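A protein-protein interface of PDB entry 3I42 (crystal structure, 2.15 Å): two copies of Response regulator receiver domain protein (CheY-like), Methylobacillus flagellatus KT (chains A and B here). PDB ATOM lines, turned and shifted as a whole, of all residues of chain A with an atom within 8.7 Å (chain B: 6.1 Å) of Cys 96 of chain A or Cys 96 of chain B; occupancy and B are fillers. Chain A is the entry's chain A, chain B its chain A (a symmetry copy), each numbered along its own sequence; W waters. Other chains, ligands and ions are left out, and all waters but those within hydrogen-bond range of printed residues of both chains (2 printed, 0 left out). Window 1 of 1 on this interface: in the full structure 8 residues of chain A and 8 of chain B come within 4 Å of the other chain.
SG of Cys 96 of chain B forms a disulfide with SG of Cys 96 of chain A (2.1 Å). The backbone carbonyl oxygen of Leu 91 of chain A sits close to the backbone carbonyl oxygen of Leu 91 of chain B (2.3 Å).
NZ of Lys 93 of chain A is in salt-bridge range of OE2 of Glu 97 of chain A (2.8 Å). The backbone carbonyl oxygen (O) of Cys 96 of chain A is in hydrogen-bond range of the side-chain hydroxyl (OH) of Tyr 102 of chain A (2.6 Å). OH of Tyr 102 of chain A sits at hydrogen-bond distance from O of Phe 99 of chain A, 3.1 Å away. NZ of Lys 93 of chain B lies within salt-bridge range of OE2 of Glu 97 of chain B, 2.8 Å away. O of Cys 96 of chain B is in hydrogen-bond range of OH of Tyr 102 of chain B, 2.7 Å away. The backbone carbonyl oxygen (O) of Phe 99 of chain B lies within hydrogen-bond range of the side-chain hydroxyl (OH) of Tyr 102 of chain B.
Among the printed residues, merely in contact across the chains: Lys 88 of chain A with Leu 91 of chain B, Lys 88 of chain A with Gly 92 of chain B, Leu 91 of chain A with Lys 93 of chain B, Leu 91 of chain A with Cys 96 of chain B, Lys 93 of chain A with Leu 91 of chain B, Lys 93 of chain A with Tyr 102 of chain B, Cys 96 of chain A with Leu 91 of chain B, Cys 96 of chain A with Tyr 102 of chain B, Glu 97 of chain A with Tyr 102 of chain B, Tyr 102 of chain A with Lys 93 of chain B, Tyr 102 of chain A with Cys 96 of chain B, Tyr 102 of chain A with Glu 97 of chain B and Tyr 102 of chain A with Tyr 102 of chain B.
Of the printed residues of chain B, Cys 96 of chain A touches Leu 91, Cys 96 and Tyr 102. Of the printed residues of chain A, Cys 96 of chain B touches Leu 91, Cys 96 and Tyr 102. Of the printed residues of chain A, Leu 91 of chain B touches Lys 88, Leu 91, Lys 93 and Cys 96. Of the printed residues of chain B, Lys 88 of chain A touches Leu 91 (3.8 Å) and Gly 92 (3.6 Å). Glu 94 of chain B touches none of the printed residues of chain A. Asp 90 of chain A touches none of the printed residues of chain B. The nearest printed residue of chain B that does not touch Cys 96 of chain A is Gly 92 of chain B (4.5 Å). The nearest printed residue of chain A that does not touch Tyr 102 of chain B is Phe 99 of chain A (6.3 Å).
Hydrophobic or aromatic side chains of chain A within 4 Å of the printed part of chain B: Leu 91 and Tyr 102. Printed residues of chain B that touch a printed residue of chain A: Leu 91, Gly 92, Lys 93, Cys 96, Glu 97 and Tyr 102. Among the printed residues, no Asp or Glu carboxylate lies within 4 Å of a Lys or Arg side-chain nitrogen of the other chain.
Leu 91 of chain A touches Lys 93 of chain B, and with the chains exchanged Lys 93 of chain A touches Leu 91 of chain B. Lys 93 of chain A touches Tyr 102 of chain B, and with the chains exchanged Tyr 102 of chain A touches Lys 93 of chain B. Cys 96 of chain B touches its own counterpart, Cys 96 of chain A. Glu 97 of chain A touches Tyr 102 of chain B, and with the chains exchanged Tyr 102 of chain A touches Glu 97 of chain B. Positions printed for both chains: 91, 92, 93, 94, 95, 96, 97, 98, 99, 100 and 102.
Water W2 bridges the side-chain carboxylate (OE2) of Glu 97 of chain B (2.7 Å) and the backbone NH (N) of Tyr 102 of chain A (3.1 Å). Water W1 lies within hydrogen-bond range of the side-chain carboxylate of Glu 97 of chain A (2.7 Å) and the backbone NH of Tyr 102 of chain B (3.1 Å).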
ATOM      1  N   LEU A  55      -4.973 -18.507 -20.555  1.00  0.00           N
ATOM      2  CA  LEU A  55      -3.942 -19.241 -19.844  1.00  0.00           C
ATOM      3  C   LEU A  55      -4.114 -20.754 -20.004  1.00  0.00           C
ATOM      4  O   LEU A  55      -3.202 -21.525 -19.660  1.00  0.00           O
ATOM      5  CB  LEU A  55      -3.872 -18.831 -18.369  1.00  0.00           C
ATOM      6  CG  LEU A  55      -3.386 -17.422 -18.066  1.00  0.00           C
ATOM      7  CD1 LEU A  55      -3.219 -17.237 -16.562  1.00  0.00           C
ATOM      8  CD2 LEU A  55      -2.081 -17.067 -18.763  1.00  0.00           C
ATOM      9  N   LEU A  63       1.345 -19.467 -20.022  1.00  0.00           N
ATOM     10  CA  LEU A  63       2.670 -19.109 -19.546  1.00  0.00           C
ATOM     11  C   LEU A  63       3.824 -19.637 -20.424  1.00  0.00           C
ATOM     12  O   LEU A  63       4.726 -18.888 -20.763  1.00  0.00           O
ATOM     13  CB  LEU A  63       2.876 -19.554 -18.091  1.00  0.00           C
ATOM     14  CG  LEU A  63       4.298 -19.153 -17.635  1.00  0.00           C
ATOM     15  CD1 LEU A  63       4.326 -17.694 -17.198  1.00  0.00           C
ATOM     16  CD2 LEU A  63       4.855 -20.097 -16.528  1.00  0.00           C
ATOM     17  N   VAL A  66       3.793 -17.497 -23.680  1.00  0.00           N
ATOM     18  CA  VAL A  66       4.273 -16.108 -23.703  1.00  0.00           C
ATOM     19  C   VAL A  66       5.825 -16.069 -23.699  1.00  0.00           C
ATOM     20  O   VAL A  66       6.426 -15.213 -24.331  1.00  0.00           O
ATOM     21  CB  VAL A  66       3.664 -15.256 -22.575  1.00  0.00           C
ATOM     22  CG1 VAL A  66       4.231 -15.634 -21.263  1.00  0.00           C
ATOM     23  CG2 VAL A  66       3.912 -13.760 -22.834  1.00  0.00           C
ATOM     24  N   ARG A  70       7.726 -13.940 -26.664  1.00  0.00           N
ATOM     25  CA  ARG A  70       8.704 -12.922 -26.292  1.00  0.00           C
ATOM     26  C   ARG A  70      10.076 -13.140 -26.937  1.00  0.00           C
ATOM     27  O   ARG A  70      10.818 -12.178 -27.171  1.00  0.00           O
ATOM     28  CB  ARG A  70       8.889 -12.885 -24.786  1.00  0.00           C
ATOM     29  CG  ARG A  70       7.796 -12.129 -24.040  1.00  0.00           C
ATOM     30  CD  ARG A  70       8.243 -11.796 -22.617  1.00  0.00           C
ATOM     31  NE  ARG A  70       7.189 -11.106 -21.880  1.00  0.00           N
ATOM     32  CZ  ARG A  70       6.865  -9.827 -22.058  1.00  0.00           C
ATOM     33  NH1 ARG A  70       7.507  -9.074 -22.962  1.00  0.00           N
ATOM     34  NH2 ARG A  70       5.878  -9.307 -21.343  1.00  0.00           N
ATOM     35  N   PHE A  80       1.719  -8.050 -23.667  1.00  0.00           N
ATOM     36  CA  PHE A  80       1.145  -9.385 -23.527  1.00  0.00           C
ATOM     37  C   PHE A  80       0.224  -9.362 -22.343  1.00  0.00           C
ATOM     38  O   PHE A  80       0.631  -8.917 -21.272  1.00  0.00           O
ATOM     39  CB  PHE A  80       2.249 -10.465 -23.309  1.00  0.00           C
ATOM     40  CG  PHE A  80       3.159 -10.628 -24.499  1.00  0.00           C
ATOM     41  CD1 PHE A  80       2.824 -11.480 -25.522  1.00  0.00           C
ATOM     42  CD2 PHE A  80       4.334  -9.870 -24.610  1.00  0.00           C
ATOM     43  CE1 PHE A  80       3.626 -11.587 -26.676  1.00  0.00           C
ATOM     44  CE2 PHE A  80       5.170  -9.982 -25.738  1.00  0.00           C
ATOM     45  CZ  PHE A  80       4.795 -10.842 -26.777  1.00  0.00           C
ATOM     46  N   ALA A  82      -2.519 -11.596 -19.937  1.00  0.00           N
ATOM     47  CA  ALA A  82      -2.987 -12.908 -19.486  1.00  0.00           C
ATOM     48  C   ALA A  82      -4.481 -12.845 -19.293  1.00  0.00           C
ATOM     49  O   ALA A  82      -4.987 -11.928 -18.649  1.00  0.00           O
ATOM     50  CB  ALA A  82      -2.369 -13.275 -18.158  1.00  0.00           C
ATOM     51  N   LYS A  88      -5.869 -15.983  -8.117  1.00  0.00           N
ATOM     52  CA  LYS A  88      -4.578 -16.371  -7.547  1.00  0.00           C
ATOM     53  C   LYS A  88      -4.057 -17.630  -8.228  1.00  0.00           C
ATOM     54  O   LYS A  88      -2.877 -17.709  -8.609  1.00  0.00           O
ATOM     55  CB  LYS A  88      -4.682 -16.589  -6.027  1.00  0.00           C
ATOM     56  N   ASP A  90      -4.048 -19.191 -10.986  1.00  0.00           N
ATOM     57  CA  ASP A  90      -3.424 -19.270 -12.304  1.00  0.00           C
ATOM     58  C   ASP A  90      -2.183 -18.362 -12.477  1.00  0.00           C
ATOM     59  O   ASP A  90      -1.340 -18.630 -13.350  1.00  0.00           O
ATOM     60  CB  ASP A  90      -4.475 -19.026 -13.405  1.00  0.00           C
ATOM     61  N   LEU A  91      -2.049 -17.321 -11.641  1.00  0.00           N
ATOM     62  CA  LEU A  91      -0.942 -16.355 -11.786  1.00  0.00           C
ATOM     63  C   LEU A  91       0.078 -16.455 -10.673  1.00  0.00           C
ATOM     64  O   LEU A  91      -0.110 -15.881  -9.609  1.00  0.00           O
ATOM     65  CB  LEU A  91      -1.463 -14.921 -11.827  1.00  0.00           C
ATOM     66  CG  LEU A  91      -2.489 -14.551 -12.888  1.00  0.00           C
ATOM     67  CD1 LEU A  91      -3.195 -13.314 -12.439  1.00  0.00           C
ATOM     68  CD2 LEU A  91      -1.833 -14.326 -14.232  1.00  0.00           C
ATOM     69  N   GLY A  92       1.167 -17.164 -10.910  1.00  0.00           N
ATOM     70  CA  GLY A  92       2.245 -17.169  -9.943  1.00  0.00           C
ATOM     71  C   GLY A  92       3.276 -16.106 -10.235  1.00  0.00           C
ATOM     72  O   GLY A  92       3.022 -15.134 -10.954  1.00  0.00           O
ATOM     73  N   LYS A  93       4.458 -16.310  -9.675  1.00  0.00           N
ATOM     74  CA  LYS A  93       5.592 -15.401  -9.800  1.00  0.00           C
ATOM     75  C   LYS A  93       6.021 -15.073 -11.245  1.00  0.00           C
ATOM     76  O   LYS A  93       6.232 -13.907 -11.578  1.00  0.00           O
ATOM     77  CB  LYS A  93       6.768 -16.002  -9.030  1.00  0.00           C
ATOM     78  CG  LYS A  93       7.972 -15.150  -9.028  1.00  0.00           C
ATOM     79  CD  LYS A  93       9.042 -15.789  -8.192  1.00  0.00           C
ATOM     80  CE  LYS A  93      10.259 -14.902  -8.206  1.00  0.00           C
ATOM     81  NZ  LYS A  93      10.768 -14.747  -9.593  1.00  0.00           N
ATOM     82  N   GLU A  94       6.187 -16.113 -12.069  1.00  0.00           N
ATOM     83  CA  GLU A  94       6.597 -15.972 -13.475  1.00  0.00           C
ATOM     84  C   GLU A  94       5.522 -15.306 -14.342  1.00  0.00           C
ATOM     85  O   GLU A  94       5.840 -14.546 -15.237  1.00  0.00           O
ATOM     86  CB  GLU A  94       6.991 -17.334 -14.077  1.00  0.00           C
ATOM     87  CG  GLU A  94       8.473 -17.705 -13.913  1.00  0.00           C
ATOM     88  CD  GLU A  94       9.014 -18.534 -15.096  1.00  0.00           C
ATOM     89  OE1 GLU A  94       8.441 -19.638 -15.355  1.00  0.00           O
ATOM     90  OE2 GLU A  94       9.996 -18.075 -15.763  1.00  0.00           O
ATOM     91  N   ALA A  95       4.256 -15.596 -14.063  1.00  0.00           N
ATOM     92  CA  ALA A  95       3.141 -14.941 -14.763  1.00  0.00           C
ATOM     93  C   ALA A  95       3.107 -13.435 -14.490  1.00  0.00           C
ATOM     94  O   ALA A  95       2.990 -12.633 -15.406  1.00  0.00           O
ATOM     95  CB  ALA A  95       1.813 -15.598 -14.407  1.00  0.00           C
ATOM     96  N   CYS A  96       3.223 -13.056 -13.225  1.00  0.00           N
ATOM     97  CA  CYS A  96       3.455 -11.658 -12.856  1.00  0.00           C
ATOM     98  C   CYS A  96       4.617 -11.033 -13.645  1.00  0.00           C
ATOM     99  O   CYS A  96       4.516  -9.901 -14.141  1.00  0.00           O
ATOM    100  CB  CYS A  96       3.719 -11.557 -11.356  1.00  0.00           C
ATOM    101  SG  CYS A  96       2.279 -11.918 -10.304  1.00  0.00           S
ATOM    102  N   GLU A  97       5.704 -11.784 -13.816  1.00  0.00           N
ATOM    103  CA  GLU A  97       6.888 -11.215 -14.460  1.00  0.00           C
ATOM    104  C   GLU A  97       6.764 -11.112 -15.972  1.00  0.00           C
ATOM    105  O   GLU A  97       7.231 -10.138 -16.558  1.00  0.00           O
ATOM    106  CB  GLU A  97       8.136 -11.994 -14.060  1.00  0.00           C
ATOM    107  CG  GLU A  97       8.419 -11.890 -12.564  1.00  0.00           C
ATOM    108  CD  GLU A  97       9.544 -12.776 -12.100  1.00  0.00           C
ATOM    109  OE1 GLU A  97       9.768 -13.806 -12.757  1.00  0.00           O
ATOM    110  OE2 GLU A  97      10.196 -12.449 -11.080  1.00  0.00           O
ATOM    111  N   LEU A  98       6.141 -12.107 -16.595  1.00  0.00           N
ATOM    112  CA  LEU A  98       6.154 -12.236 -18.067  1.00  0.00           C
ATOM    113  C   LEU A  98       4.967 -11.628 -18.812  1.00  0.00           C
ATOM    114  O   LEU A  98       5.024 -11.452 -20.040  1.00  0.00           O
ATOM    115  CB  LEU A  98       6.273 -13.708 -18.445  1.00  0.00           C
ATOM    116  CG  LEU A  98       7.619 -14.390 -18.213  1.00  0.00           C
ATOM    117  CD1 LEU A  98       7.376 -15.852 -17.935  1.00  0.00           C
ATOM    118  CD2 LEU A  98       8.509 -14.195 -19.433  1.00  0.00           C
ATOM    119  N   PHE A  99       3.879 -11.334 -18.100  1.00  0.00           N
ATOM    120  CA  PHE A  99       2.777 -10.596 -18.749  1.00  0.00           C
ATOM    121  C   PHE A  99       2.805  -9.147 -18.313  1.00  0.00           C
ATOM    122  O   PHE A  99       3.289  -8.822 -17.239  1.00  0.00           O
ATOM    123  CB  PHE A  99       1.435 -11.187 -18.398  1.00  0.00           C
ATOM    124  CG  PHE A  99       1.169 -12.494 -19.024  1.00  0.00           C
ATOM    125  CD1 PHE A  99       0.640 -12.567 -20.313  1.00  0.00           C
ATOM    126  CD2 PHE A  99       1.404 -13.666 -18.317  1.00  0.00           C
ATOM    127  CE1 PHE A  99       0.371 -13.799 -20.907  1.00  0.00           C
ATOM    128  CE2 PHE A  99       1.149 -14.914 -18.904  1.00  0.00           C
ATOM    129  CZ  PHE A  99       0.624 -14.983 -20.200  1.00  0.00           C
ATOM    130  N   ASP A 100       2.288  -8.272 -19.157  1.00  0.00           N
ATOM    131  CA  ASP A 100       2.261  -6.852 -18.853  1.00  0.00           C
ATOM    132  C   ASP A 100       0.929  -6.443 -18.208  1.00  0.00           C
ATOM    133  O   ASP A 100       0.891  -5.511 -17.404  1.00  0.00           O
ATOM    134  CB  ASP A 100       2.505  -6.063 -20.146  1.00  0.00           C
ATOM    135  CG  ASP A 100       3.825  -6.435 -20.821  1.00  0.00           C
ATOM    136  OD1 ASP A 100       4.889  -6.170 -20.227  1.00  0.00           O
ATOM    137  OD2 ASP A 100       3.791  -6.995 -21.937  1.00  0.00           O
ATOM    138  N   PHE A 101      -0.146  -7.132 -18.584  1.00  0.00           N
ATOM    139  CA  PHE A 101      -1.496  -6.838 -18.091  1.00  0.00           C
ATOM    140  C   PHE A 101      -2.218  -8.136 -17.853  1.00  0.00           C
ATOM    141  O   PHE A 101      -1.869  -9.175 -18.392  1.00  0.00           O
ATOM    142  CB  PHE A 101      -2.313  -5.971 -19.091  1.00  0.00           C
ATOM    143  CG  PHE A 101      -1.607  -4.716 -19.544  1.00  0.00           C
ATOM    144  CD1 PHE A 101      -1.684  -3.545 -18.805  1.00  0.00           C
ATOM    145  CD2 PHE A 101      -0.861  -4.709 -20.712  1.00  0.00           C
ATOM    146  CE1 PHE A 101      -1.013  -2.405 -19.223  1.00  0.00           C
ATOM    147  CE2 PHE A 101      -0.200  -3.552 -21.151  1.00  0.00           C
ATOM    148  CZ  PHE A 101      -0.268  -2.414 -20.412  1.00  0.00           C
ATOM    149  N   TYR A 102      -3.247  -8.078 -17.032  1.00  0.00           N
ATOM    150  CA  TYR A 102      -3.910  -9.278 -16.594  1.00  0.00           C
ATOM    151  C   TYR A 102      -5.407  -8.986 -16.629  1.00  0.00           C
ATOM    152  O   TYR A 102      -5.821  -7.923 -16.219  1.00  0.00           O
ATOM    153  CB  TYR A 102      -3.415  -9.677 -15.178  1.00  0.00           C
ATOM    154  CG  TYR A 102      -1.920  -9.440 -14.950  1.00  0.00           C
ATOM    155  CD1 TYR A 102      -0.959 -10.481 -15.117  1.00  0.00           C
ATOM    156  CD2 TYR A 102      -1.457  -8.183 -14.573  1.00  0.00           C
ATOM    157  CE1 TYR A 102       0.442 -10.240 -14.903  1.00  0.00           C
ATOM    158  CE2 TYR A 102      -0.079  -7.935 -14.382  1.00  0.00           C
ATOM    159  CZ  TYR A 102       0.852  -8.963 -14.543  1.00  0.00           C
ATOM    160  OH  TYR A 102       2.181  -8.663 -14.334  1.00  0.00           O
ATOM    161  N   LEU A 103      -6.181  -9.929 -17.168  1.00  0.00           N
ATOM    162  CA  LEU A 103      -7.634  -9.869 -17.296  1.00  0.00           C
ATOM    163  C   LEU A 103      -8.225 -11.098 -16.647  1.00  0.00           C
ATOM    164  O   LEU A 103      -7.662 -12.189 -16.718  1.00  0.00           O
ATOM    165  CB  LEU A 103      -8.034  -9.891 -18.774  1.00  0.00           C
ATOM    166  CG  LEU A 103      -7.932  -8.572 -19.516  1.00  0.00           C
ATOM    167  CD1 LEU A 103      -8.170  -8.798 -20.989  1.00  0.00           C
ATOM    168  CD2 LEU A 103      -8.968  -7.588 -18.946  1.00  0.00           C
ATOM    169  N   LEU B  91       0.275 -14.734  -4.953  1.00  0.00           N
ATOM    170  CA  LEU B  91       0.235 -13.663  -5.967  1.00  0.00           C
ATOM    171  C   LEU B  91      -0.915 -13.811  -6.940  1.00  0.00           C
ATOM    172  O   LEU B  91      -0.813 -14.548  -7.910  1.00  0.00           O
ATOM    173  CB  LEU B  91       1.533 -13.613  -6.770  1.00  0.00           C
ATOM    174  CG  LEU B  91       2.845 -13.437  -6.019  1.00  0.00           C
ATOM    175  CD1 LEU B  91       3.952 -13.908  -6.905  1.00  0.00           C
ATOM    176  CD2 LEU B  91       3.062 -11.994  -5.624  1.00  0.00           C
ATOM    177  N   GLY B  92      -2.007 -13.107  -6.699  1.00  0.00           N
ATOM    178  CA  GLY B  92      -3.079 -13.090  -7.673  1.00  0.00           C
ATOM    179  C   GLY B  92      -2.951 -11.938  -8.640  1.00  0.00           C
ATOM    180  O   GLY B  92      -1.879 -11.348  -8.809  1.00  0.00           O
ATOM    181  N   LYS B  93      -4.070 -11.615  -9.268  1.00  0.00           N
ATOM    182  CA  LYS B  93      -4.172 -10.553 -10.264  1.00  0.00           C
ATOM    183  C   LYS B  93      -3.700  -9.160  -9.798  1.00  0.00           C
ATOM    184  O   LYS B  93      -2.951  -8.492 -10.509  1.00  0.00           O
ATOM    185  CB  LYS B  93      -5.625 -10.483 -10.732  1.00  0.00           C
ATOM    186  CG  LYS B  93      -5.859  -9.480 -11.789  1.00  0.00           C
ATOM    187  CD  LYS B  93      -7.292  -9.535 -12.230  1.00  0.00           C
ATOM    188  CE  LYS B  93      -7.506  -8.504 -13.308  1.00  0.00           C
ATOM    189  NZ  LYS B  93      -7.221  -7.144 -12.782  1.00  0.00           N
ATOM    190  N   GLU B  94      -4.184  -8.727  -8.629  1.00  0.00           N
ATOM    191  CA  GLU B  94      -3.837  -7.421  -8.046  1.00  0.00           C
ATOM    192  C   GLU B  94      -2.371  -7.342  -7.603  1.00  0.00           C
ATOM    193  O   GLU B  94      -1.748  -6.304  -7.731  1.00  0.00           O
ATOM    194  CB  GLU B  94      -4.764  -7.079  -6.864  1.00  0.00           C
ATOM    195  CG  GLU B  94      -6.041  -6.318  -7.250  1.00  0.00           C
ATOM    196  CD  GLU B  94      -6.498  -5.329  -6.158  1.00  0.00           C
ATOM    197  OE1 GLU B  94      -6.750  -5.799  -5.004  1.00  0.00           O
ATOM    198  OE2 GLU B  94      -6.595  -4.094  -6.453  1.00  0.00           O
ATOM    199  N   ALA B  95      -1.834  -8.443  -7.090  1.00  0.00           N
ATOM    200  CA  ALA B  95      -0.410  -8.509  -6.725  1.00  0.00           C
ATOM    201  C   ALA B  95       0.497  -8.348  -7.947  1.00  0.00           C
ATOM    202  O   ALA B  95       1.441  -7.570  -7.930  1.00  0.00           O
ATOM    203  CB  ALA B  95      -0.101  -9.800  -5.973  1.00  0.00           C
ATOM    204  N   CYS B  96       0.198  -9.077  -9.012  1.00  0.00           N
ATOM    205  CA  CYS B  96       0.824  -8.835 -10.313  1.00  0.00           C
ATOM    206  C   CYS B  96       0.764  -7.354 -10.723  1.00  0.00           C
ATOM    207  O   CYS B  96       1.757  -6.782 -11.196  1.00  0.00           O
ATOM    208  CB  CYS B  96       0.157  -9.704 -11.377  1.00  0.00           C
ATOM    209  SG  CYS B  96       0.476 -11.488 -11.209  1.00  0.00           S
ATOM    210  N   GLU B  97      -0.378  -6.710 -10.491  1.00  0.00           N
ATOM    211  CA  GLU B  97      -0.543  -5.331 -10.954  1.00  0.00           C
ATOM    212  C   GLU B  97       0.169  -4.310 -10.082  1.00  0.00           C
ATOM    213  O   GLU B  97       0.719  -3.341 -10.601  1.00  0.00           O
ATOM    214  CB  GLU B  97      -2.022  -4.994 -11.104  1.00  0.00           C
ATOM    215  CG  GLU B  97      -2.698  -5.849 -12.173  1.00  0.00           C
ATOM    216  CD  GLU B  97      -4.191  -5.664 -12.237  1.00  0.00           C
ATOM    217  OE1 GLU B  97      -4.768  -5.309 -11.196  1.00  0.00           O
ATOM    218  OE2 GLU B  97      -4.785  -5.881 -13.320  1.00  0.00           O
ATOM    219  N   LEU B  98       0.159  -4.525  -8.771  1.00  0.00           N
ATOM    220  CA  LEU B  98       0.615  -3.501  -7.808  1.00  0.00           C
ATOM    221  C   LEU B  98       2.070  -3.596  -7.356  1.00  0.00           C
ATOM    222  O   LEU B  98       2.606  -2.640  -6.770  1.00  0.00           O
ATOM    223  CB  LEU B  98      -0.288  -3.525  -6.580  1.00  0.00           C
ATOM    224  CG  LEU B  98      -1.705  -2.980  -6.733  1.00  0.00           C
ATOM    225  CD1 LEU B  98      -2.608  -3.705  -5.767  1.00  0.00           C
ATOM    226  CD2 LEU B  98      -1.708  -1.479  -6.478  1.00  0.00           C
ATOM    227  N   PHE B  99       2.712  -4.742  -7.582  1.00  0.00           N
ATOM    228  CA  PHE B  99       4.162  -4.815  -7.311  1.00  0.00           C
ATOM    229  C   PHE B  99       4.931  -4.742  -8.613  1.00  0.00           C
ATOM    230  O   PHE B  99       4.425  -5.109  -9.664  1.00  0.00           O
ATOM    231  CB  PHE B  99       4.525  -6.094  -6.600  1.00  0.00           C
ATOM    232  CG  PHE B  99       4.076  -6.152  -5.197  1.00  0.00           C
ATOM    233  CD1 PHE B  99       4.857  -5.599  -4.181  1.00  0.00           C
ATOM    234  CD2 PHE B  99       2.891  -6.796  -4.870  1.00  0.00           C
ATOM    235  CE1 PHE B  99       4.447  -5.663  -2.850  1.00  0.00           C
ATOM    236  CE2 PHE B  99       2.459  -6.860  -3.537  1.00  0.00           C
ATOM    237  CZ  PHE B  99       3.242  -6.299  -2.521  1.00  0.00           C
ATOM    238  N   ASP B 100       6.158  -4.260  -8.540  1.00  0.00           N
ATOM    239  CA  ASP B 100       6.993  -4.137  -9.723  1.00  0.00           C
ATOM    240  C   ASP B 100       7.896  -5.366  -9.901  1.00  0.00           C
ATOM    241  O   ASP B 100       8.232  -5.729 -11.029  1.00  0.00           O
ATOM    242  CB  ASP B 100       7.832  -2.857  -9.606  1.00  0.00           C
ATOM    243  CG  ASP B 100       6.973  -1.605  -9.432  1.00  0.00           C
ATOM    244  OD1 ASP B 100       6.226  -1.265 -10.371  1.00  0.00           O
ATOM    245  OD2 ASP B 100       7.044  -0.974  -8.356  1.00  0.00           O
ATOM    246  N   TYR B 102       9.129  -9.352  -7.880  1.00  0.00           N
ATOM    247  CA  TYR B 102       8.616 -10.401  -7.039  1.00  0.00           C
ATOM    248  C   TYR B 102       9.803 -11.284  -6.669  1.00  0.00           C
ATOM    249  O   TYR B 102      10.619 -11.579  -7.515  1.00  0.00           O
ATOM    250  CB  TYR B 102       7.500 -11.185  -7.783  1.00  0.00           C
ATOM    251  CG  TYR B 102       6.589 -10.308  -8.645  1.00  0.00           C
ATOM    252  CD1 TYR B 102       5.338  -9.822  -8.161  1.00  0.00           C
ATOM    253  CD2 TYR B 102       6.968  -9.956  -9.936  1.00  0.00           C
ATOM    254  CE1 TYR B 102       4.495  -8.995  -8.983  1.00  0.00           C
ATOM    255  CE2 TYR B 102       6.154  -9.126 -10.740  1.00  0.00           C
ATOM    256  CZ  TYR B 102       4.929  -8.661 -10.259  1.00  0.00           C
ATOM    257  OH  TYR B 102       4.175  -7.863 -11.092  1.00  0.00           O
HETATM  258  O   HOH W   1      10.597  -9.775 -10.608  1.00  0.00           O
HETATM  259  O   HOH W   2      -3.471  -5.280 -15.654  1.00  0.00           O
